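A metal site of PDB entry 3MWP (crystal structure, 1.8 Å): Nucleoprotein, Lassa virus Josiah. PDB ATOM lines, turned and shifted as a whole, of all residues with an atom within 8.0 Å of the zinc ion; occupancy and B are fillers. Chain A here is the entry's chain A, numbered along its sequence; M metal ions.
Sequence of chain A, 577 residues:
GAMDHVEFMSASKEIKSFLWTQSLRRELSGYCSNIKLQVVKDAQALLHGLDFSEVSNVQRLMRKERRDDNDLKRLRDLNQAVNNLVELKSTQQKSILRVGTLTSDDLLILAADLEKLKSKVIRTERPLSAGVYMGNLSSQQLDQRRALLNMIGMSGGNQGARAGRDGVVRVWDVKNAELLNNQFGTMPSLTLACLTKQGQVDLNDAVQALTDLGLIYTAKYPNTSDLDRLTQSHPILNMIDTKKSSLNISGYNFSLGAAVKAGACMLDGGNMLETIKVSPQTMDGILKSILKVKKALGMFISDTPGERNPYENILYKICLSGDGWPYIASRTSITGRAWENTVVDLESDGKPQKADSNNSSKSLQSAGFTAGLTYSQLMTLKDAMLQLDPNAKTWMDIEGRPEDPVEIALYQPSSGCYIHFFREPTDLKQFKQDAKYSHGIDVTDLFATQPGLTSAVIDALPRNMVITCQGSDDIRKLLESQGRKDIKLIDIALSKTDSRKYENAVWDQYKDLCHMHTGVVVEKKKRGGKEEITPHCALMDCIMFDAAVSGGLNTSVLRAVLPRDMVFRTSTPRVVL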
ATOM      1  N   GLU A 399      21.957  11.480  -2.696  1.00  0.00           N
ATOM      2  CA  GLU A 399      22.251  12.214  -1.444  1.00  0.00           C
ATOM      3  C   GLU A 399      21.969  11.315  -0.252  1.00  0.00           C
ATOM      4  O   GLU A 399      21.037  10.515  -0.285  1.00  0.00           O
ATOM      5  CB  GLU A 399      21.427  13.497  -1.322  1.00  0.00           C
ATOM      6  CG  GLU A 399      21.955  14.638  -2.185  1.00  0.00           C
ATOM      7  CD  GLU A 399      23.346  15.084  -1.772  1.00  0.00           C
ATOM      8  OE1 GLU A 399      23.559  15.264  -0.563  1.00  0.00           O
ATOM      9  OE2 GLU A 399      24.209  15.270  -2.640  1.00  0.00           O
ATOM     10  N   GLU A 407      17.897  10.771  -1.251  1.00  0.00           N
ATOM     11  CA  GLU A 407      17.501  11.287  -2.561  1.00  0.00           C
ATOM     12  C   GLU A 407      18.276  10.587  -3.661  1.00  0.00           C
ATOM     13  O   GLU A 407      19.489  10.445  -3.571  1.00  0.00           O
ATOM     14  CB  GLU A 407      17.668  12.814  -2.622  1.00  0.00           C
ATOM     15  CG  GLU A 407      17.172  13.413  -3.964  1.00  0.00           C
ATOM     16  CD  GLU A 407      17.459  14.932  -4.067  1.00  0.00           C
ATOM     17  OE1 GLU A 407      18.576  15.380  -3.737  1.00  0.00           O
ATOM     18  OE2 GLU A 407      16.590  15.637  -4.543  1.00  0.00           O
ATOM     19  N   ILE A 408      17.549  10.093  -4.663  1.00  0.00           N
ATOM     20  CA  ILE A 408      18.121   9.340  -5.777  1.00  0.00           C
ATOM     21  C   ILE A 408      17.680   9.958  -7.086  1.00  0.00           C
ATOM     22  O   ILE A 408      16.504  10.264  -7.244  1.00  0.00           O
ATOM     23  CB  ILE A 408      17.642   7.851  -5.814  1.00  0.00           C
ATOM     24  CG1 ILE A 408      17.879   7.133  -4.483  1.00  0.00           C
ATOM     25  CG2 ILE A 408      18.260   7.102  -7.041  1.00  0.00           C
ATOM     26  CD1 ILE A 408      19.238   7.231  -3.991  1.00  0.00           C
ATOM     27  N   ALA A 409      18.606  10.095  -8.022  1.00  0.00           N
ATOM     28  CA  ALA A 409      18.231  10.574  -9.356  1.00  0.00           C
ATOM     29  C   ALA A 409      19.005   9.861 -10.436  1.00  0.00           C
ATOM     30  O   ALA A 409      20.196   9.548 -10.253  1.00  0.00           O
ATOM     31  CB  ALA A 409      18.411  12.090  -9.466  1.00  0.00           C
ATOM     32  N   HIS A 420      13.593  10.563 -10.306  1.00  0.00           N
ATOM     33  CA  HIS A 420      13.959  11.319  -9.104  1.00  0.00           C
ATOM     34  C   HIS A 420      12.975  11.004  -7.982  1.00  0.00           C
ATOM     35  O   HIS A 420      11.752  11.085  -8.184  1.00  0.00           O
ATOM     36  CB  HIS A 420      14.006  12.832  -9.450  1.00  0.00           C
ATOM     37  CG  HIS A 420      14.202  13.749  -8.286  1.00  0.00           C
ATOM     38  ND1 HIS A 420      13.441  14.885  -8.103  1.00  0.00           N
ATOM     39  CD2 HIS A 420      15.089  13.723  -7.270  1.00  0.00           C
ATOM     40  CE1 HIS A 420      13.851  15.518  -7.018  1.00  0.00           C
ATOM     41  NE2 HIS A 420      14.839  14.829  -6.488  1.00  0.00           N
ATOM     42  N   PHE A 421      13.491  10.543  -6.828  1.00  0.00           N
ATOM     43  CA  PHE A 421      12.644  10.197  -5.679  1.00  0.00           C
ATOM     44  C   PHE A 421      13.415  10.250  -4.382  1.00  0.00           C
ATOM     45  O   PHE A 421      14.644  10.473  -4.367  1.00  0.00           O
ATOM     46  CB  PHE A 421      11.968   8.826  -5.861  1.00  0.00           C
ATOM     47  CG  PHE A 421      12.945   7.709  -5.963  1.00  0.00           C
ATOM     48  CD1 PHE A 421      13.368   7.018  -4.826  1.00  0.00           C
ATOM     49  CD2 PHE A 421      13.488   7.363  -7.196  1.00  0.00           C
ATOM     50  CE1 PHE A 421      14.281   5.978  -4.925  1.00  0.00           C
ATOM     51  CE2 PHE A 421      14.429   6.325  -7.312  1.00  0.00           C
ATOM     52  CZ  PHE A 421      14.801   5.608  -6.163  1.00  0.00           C
ATOM     53  N   PHE A 422      12.688  10.069  -3.292  1.00  0.00           N
ATOM     54  CA  PHE A 422      13.252  10.292  -1.983  1.00  0.00           C
ATOM     55  C   PHE A 422      13.075   9.074  -1.094  1.00  0.00           C
ATOM     56  O   PHE A 422      12.335   8.158  -1.430  1.00  0.00           O
ATOM     57  CB  PHE A 422      12.577  11.470  -1.327  1.00  0.00           C
ATOM     58  CG  PHE A 422      12.630  12.716  -2.154  1.00  0.00           C
ATOM     59  CD1 PHE A 422      13.737  13.555  -2.071  1.00  0.00           C
ATOM     60  CD2 PHE A 422      11.590  13.050  -2.999  1.00  0.00           C
ATOM     61  CE1 PHE A 422      13.828  14.717  -2.827  1.00  0.00           C
ATOM     62  CE2 PHE A 422      11.652  14.245  -3.774  1.00  0.00           C
ATOM     63  CZ  PHE A 422      12.793  15.081  -3.677  1.00  0.00           C
ATOM     64  N   HIS A 439      22.924  18.541   1.786  1.00  0.00           N
ATOM     65  CA  HIS A 439      21.669  18.547   1.042  1.00  0.00           C
ATOM     66  C   HIS A 439      20.558  19.483   1.525  1.00  0.00           C
ATOM     67  O   HIS A 439      19.608  19.775   0.770  1.00  0.00           O
ATOM     68  CB  HIS A 439      21.110  17.116   0.818  1.00  0.00           C
ATOM     69  CG  HIS A 439      20.904  16.311   2.078  1.00  0.00           C
ATOM     70  ND1 HIS A 439      20.109  16.747   3.118  1.00  0.00           N
ATOM     71  CD2 HIS A 439      21.298  15.056   2.403  1.00  0.00           C
ATOM     72  CE1 HIS A 439      20.097  15.827   4.062  1.00  0.00           C
ATOM     73  NE2 HIS A 439      20.800  14.786   3.653  1.00  0.00           N
ATOM     74  N   ILE A 441      18.114  19.042   3.504  1.00  0.00           N
ATOM     75  CA  ILE A 441      16.777  18.461   3.611  1.00  0.00           C
ATOM     76  C   ILE A 441      16.315  18.402   5.089  1.00  0.00           C
ATOM     77  O   ILE A 441      17.048  17.943   5.962  1.00  0.00           O
ATOM     78  CB  ILE A 441      16.661  17.073   2.928  1.00  0.00           C
ATOM     79  CG1 ILE A 441      17.024  17.127   1.437  1.00  0.00           C
ATOM     80  CG2 ILE A 441      15.241  16.551   3.070  1.00  0.00           C
ATOM     81  CD1 ILE A 441      17.192  15.716   0.789  1.00  0.00           C
ATOM     82  N   TRP A 507      20.375  25.395 -11.770  1.00  0.00           N
ATOM     83  CA  TRP A 507      19.328  25.796 -10.853  1.00  0.00           C
ATOM     84  C   TRP A 507      18.453  26.883 -11.496  1.00  0.00           C
ATOM     85  O   TRP A 507      17.228  26.898 -11.338  1.00  0.00           O
ATOM     86  CB  TRP A 507      19.914  26.266  -9.527  1.00  0.00           C
ATOM     87  CG  TRP A 507      20.364  25.179  -8.595  1.00  0.00           C
ATOM     88  CD1 TRP A 507      21.643  24.827  -8.345  1.00  0.00           C
ATOM     89  CD2 TRP A 507      19.533  24.333  -7.764  1.00  0.00           C
ATOM     90  NE1 TRP A 507      21.684  23.793  -7.422  1.00  0.00           N
ATOM     91  CE2 TRP A 507      20.403  23.458  -7.075  1.00  0.00           C
ATOM     92  CE3 TRP A 507      18.153  24.190  -7.598  1.00  0.00           C
ATOM     93  CZ2 TRP A 507      19.931  22.514  -6.145  1.00  0.00           C
ATOM     94  CZ3 TRP A 507      17.674  23.228  -6.671  1.00  0.00           C
ATOM     95  CH2 TRP A 507      18.582  22.392  -5.980  1.00  0.00           C
ATOM     96  N   LYS A 511      15.123  24.862 -11.297  1.00  0.00           N
ATOM     97  CA  LYS A 511      14.744  24.961  -9.892  1.00  0.00           C
ATOM     98  C   LYS A 511      13.346  24.396  -9.595  1.00  0.00           C
ATOM     99  O   LYS A 511      13.168  23.730  -8.564  1.00  0.00           O
ATOM    100  CB  LYS A 511      14.864  26.384  -9.359  1.00  0.00           C
ATOM    101  CG  LYS A 511      14.217  26.595  -7.984  1.00  0.00           C
ATOM    102  CD  LYS A 511      14.803  25.681  -6.934  1.00  0.00           C
ATOM    103  CE  LYS A 511      13.998  25.752  -5.616  1.00  0.00           C
ATOM    104  NZ  LYS A 511      12.651  25.153  -5.728  1.00  0.00           N
ATOM    105  N   LEU A 513      12.008  21.779 -10.538  1.00  0.00           N
ATOM    106  CA  LEU A 513      11.960  20.298 -10.523  1.00  0.00           C
ATOM    107  C   LEU A 513      12.224  19.674  -9.142  1.00  0.00           C
ATOM    108  O   LEU A 513      11.926  18.510  -8.918  1.00  0.00           O
ATOM    109  CB  LEU A 513      12.894  19.683 -11.561  1.00  0.00           C
ATOM    110  CG  LEU A 513      12.655  20.165 -12.991  1.00  0.00           C
ATOM    111  CD1 LEU A 513      13.508  19.349 -13.970  1.00  0.00           C
ATOM    112  CD2 LEU A 513      11.143  20.078 -13.348  1.00  0.00           C
ATOM    113  N   CYS A 514      12.783  20.450  -8.225  1.00  0.00           N
ATOM    114  CA  CYS A 514      12.930  19.946  -6.879  1.00  0.00           C
ATOM    115  C   CYS A 514      12.721  21.045  -5.843  1.00  0.00           C
ATOM    116  O   CYS A 514      13.391  22.087  -5.886  1.00  0.00           O
ATOM    117  CB  CYS A 514      14.286  19.271  -6.672  1.00  0.00           C
ATOM    118  SG  CYS A 514      14.420  18.416  -5.077  1.00  0.00           S
ATOM    119  N   HIS A 515      11.822  20.801  -4.897  1.00  0.00           N
ATOM    120  CA  HIS A 515      11.591  21.765  -3.818  1.00  0.00           C
ATOM    121  C   HIS A 515      12.002  21.246  -2.434  1.00  0.00           C
ATOM    122  O   HIS A 515      11.567  21.800  -1.434  1.00  0.00           O
ATOM    123  CB  HIS A 515      10.133  22.218  -3.777  1.00  0.00           C
ATOM    124  CG  HIS A 515       9.681  22.951  -5.006  1.00  0.00           C
ATOM    125  ND1 HIS A 515       9.227  22.305  -6.130  1.00  0.00           N
ATOM    126  CD2 HIS A 515       9.568  24.277  -5.251  1.00  0.00           C
ATOM    127  CE1 HIS A 515       8.886  23.202  -7.044  1.00  0.00           C
ATOM    128  NE2 HIS A 515       9.080  24.407  -6.530  1.00  0.00           N
ATOM    129  N   MET A 516      12.842  20.218  -2.374  1.00  0.00           N
ATOM    130  CA  MET A 516      13.148  19.537  -1.123  1.00  0.00           C
ATOM    131  C   MET A 516      14.283  20.189  -0.324  1.00  0.00           C
ATOM    132  O   MET A 516      14.443  19.908   0.878  1.00  0.00           O
ATOM    133  CB  MET A 516      13.438  18.038  -1.423  1.00  0.00           C
ATOM    134  CG  MET A 516      13.487  17.154  -0.200  1.00  0.00           C
ATOM    135  SD  MET A 516      11.937  17.032   0.726  1.00  0.00           S
ATOM    136  CE  MET A 516      10.759  16.308  -0.387  1.00  0.00           C
ATOM    137  N   HIS A 517      15.046  21.082  -0.950  1.00  0.00           N
ATOM    138  CA  HIS A 517      16.266  21.603  -0.332  1.00  0.00           C
ATOM    139  C   HIS A 517      16.006  22.976   0.275  1.00  0.00           C
ATOM    140  O   HIS A 517      15.975  23.985  -0.430  1.00  0.00           O
ATOM    141  CB  HIS A 517      17.421  21.587  -1.326  1.00  0.00           C
ATOM    142  CG  HIS A 517      17.601  20.248  -1.969  1.00  0.00           C
ATOM    143  ND1 HIS A 517      18.370  19.240  -1.418  1.00  0.00           N
ATOM    144  CD2 HIS A 517      17.058  19.731  -3.093  1.00  0.00           C
ATOM    145  CE1 HIS A 517      18.304  18.174  -2.199  1.00  0.00           C
ATOM    146  NE2 HIS A 517      17.500  18.437  -3.214  1.00  0.00           N
ATOM    147  N   PRO A 535      22.681  24.217  -1.735  1.00  0.00           N
ATOM    148  CA  PRO A 535      22.494  22.805  -1.343  1.00  0.00           C
ATOM    149  C   PRO A 535      22.714  21.874  -2.503  1.00  0.00           C
ATOM    150  O   PRO A 535      22.484  22.261  -3.652  1.00  0.00           O
ATOM    151  CB  PRO A 535      21.011  22.731  -0.944  1.00  0.00           C
ATOM    152  CG  PRO A 535      20.700  24.163  -0.433  1.00  0.00           C
ATOM    153  CD  PRO A 535      21.539  25.076  -1.332  1.00  0.00           C
ATOM    154  N   HIS A 536      23.136  20.655  -2.207  1.00  0.00           N
ATOM    155  CA  HIS A 536      23.275  19.619  -3.191  1.00  0.00           C
ATOM    156  C   HIS A 536      21.999  18.791  -3.410  1.00  0.00           C
ATOM    157  O   HIS A 536      21.423  18.260  -2.477  1.00  0.00           O
ATOM    158  CB  HIS A 536      24.439  18.709  -2.818  1.00  0.00           C
ATOM    159  CG  HIS A 536      25.739  19.431  -2.699  1.00  0.00           C
ATOM    160  ND1 HIS A 536      26.838  18.865  -2.100  1.00  0.00           N
ATOM    161  CD2 HIS A 536      26.132  20.664  -3.118  1.00  0.00           C
ATOM    162  CE1 HIS A 536      27.850  19.718  -2.137  1.00  0.00           C
ATOM    163  NE2 HIS A 536      27.450  20.811  -2.755  1.00  0.00           N
ATOM    164  N   CYS A 537      21.577  18.703  -4.666  1.00  0.00           N
ATOM    165  CA  CYS A 537      20.408  17.931  -5.092  1.00  0.00           C
ATOM    166  C   CYS A 537      20.869  16.837  -6.027  1.00  0.00           C
ATOM    167  O   CYS A 537      21.653  17.110  -6.952  1.00  0.00           O
ATOM    168  CB  CYS A 537      19.472  18.880  -5.851  1.00  0.00           C
ATOM    169  SG  CYS A 537      18.089  18.074  -6.668  1.00  0.00           S
ATOM    170  N   ALA A 538      20.413  15.603  -5.800  1.00  0.00           N
ATOM    171  CA  ALA A 538      20.840  14.481  -6.649  1.00  0.00           C
ATOM    172  C   ALA A 538      20.500  14.746  -8.111  1.00  0.00           C
ATOM    173  O   ALA A 538      21.277  14.398  -9.001  1.00  0.00           O
ATOM    174  CB  ALA A 538      20.185  13.223  -6.196  1.00  0.00           C
ATOM    175  N   LEU A 539      19.328  15.337  -8.363  1.00  0.00           N
ATOM    176  CA  LEU A 539      18.898  15.606  -9.743  1.00  0.00           C
ATOM    177  C   LEU A 539      19.749  16.694 -10.397  1.00  0.00           C
ATOM    178  O   LEU A 539      20.270  16.481 -11.488  1.00  0.00           O
ATOM    179  CB  LEU A 539      17.405  15.945  -9.827  1.00  0.00           C
ATOM    180  CG  LEU A 539      16.793  16.269 -11.198  1.00  0.00           C
ATOM    181  CD1 LEU A 539      17.084  15.149 -12.218  1.00  0.00           C
ATOM    182  CD2 LEU A 539      15.283  16.514 -11.021  1.00  0.00           C
ATOM    183  N   MET A 540      19.888  17.851  -9.730  1.00  0.00           N
ATOM    184  CA  MET A 540      20.647  18.965 -10.295  1.00  0.00           C
ATOM    185  C   MET A 540      22.100  18.548 -10.480  1.00  0.00           C
ATOM    186  O   MET A 540      22.744  18.973 -11.452  1.00  0.00           O
ATOM    187  CB  MET A 540      20.585  20.216  -9.399  1.00  0.00           C
ATOM    188  CG  MET A 540      19.158  20.776  -9.147  1.00  0.00           C
ATOM    189  SD  MET A 540      18.113  20.928 -10.646  1.00  0.00           S
ATOM    190  CE  MET A 540      16.481  20.616  -9.987  1.00  0.00           C
ATOM    191  N   ASP A 541      22.593  17.703  -9.570  1.00  0.00           N
ATOM    192  CA  ASP A 541      23.971  17.213  -9.707  1.00  0.00           C
ATOM    193  C   ASP A 541      24.121  16.395 -10.994  1.00  0.00           C
ATOM    194  O   ASP A 541      25.071  16.612 -11.736  1.00  0.00           O
ATOM    195  CB  ASP A 541      24.417  16.411  -8.510  1.00  0.00           C
ATOM    196  CG  ASP A 541      24.916  17.284  -7.365  1.00  0.00           C
ATOM    197  OD1 ASP A 541      24.986  18.531  -7.481  1.00  0.00           O
ATOM    198  OD2 ASP A 541      25.249  16.697  -6.308  1.00  0.00           O
HETATM  199 ZN    ZN M   1      16.736  17.613  -4.960  1.00  0.00          ZN
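The zinc ion is bound by the side-chain carboxylate of Glu 407 (2.0 Å), a ring nitrogen (NE2) of His 517 (2.1 Å), the side-chain sulfur of Cys 537 (2.2 Å) and the side-chain sulfur of Cys 514 (2.5 Å).
The zinc ion has four donor atoms within binding distance.
The backbone NH (N) of Glu 399 sits at hydrogen-bond distance from the backbone carbonyl oxygen (O) of Glu 407, at 2.8 Å.
SG of Cys 514 sits close to N of Met 516 (3.6 Å).
The side-chain carboxylate of Glu 407 lies close to a ring nitrogen (NE2) of His 420 (2.7 Å).
The side-chain sulfur (SG) of Cys 537 sits close to the backbone NH (N) of Met 540 (3.6 Å).
The side-chain carboxylate of Glu 407 lies within hydrogen-bond range of the backbone NH of Ala 538, 2.8 Å away.
O of His 536 lies close to ND1 of His 517, 3.4 Å away.
The backbone carbonyl oxygen (O) of Cys 514 lies within hydrogen-bond range of the side-chain amino group (NZ) of Lys 511.
N of Leu 539 sits close to SG of Cys 537, 3.4 Å away.
Merely in contact with the zinc ion: His 420.
Along chain A the residues within 4 Å of the zinc ion span positions 407 to 537.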
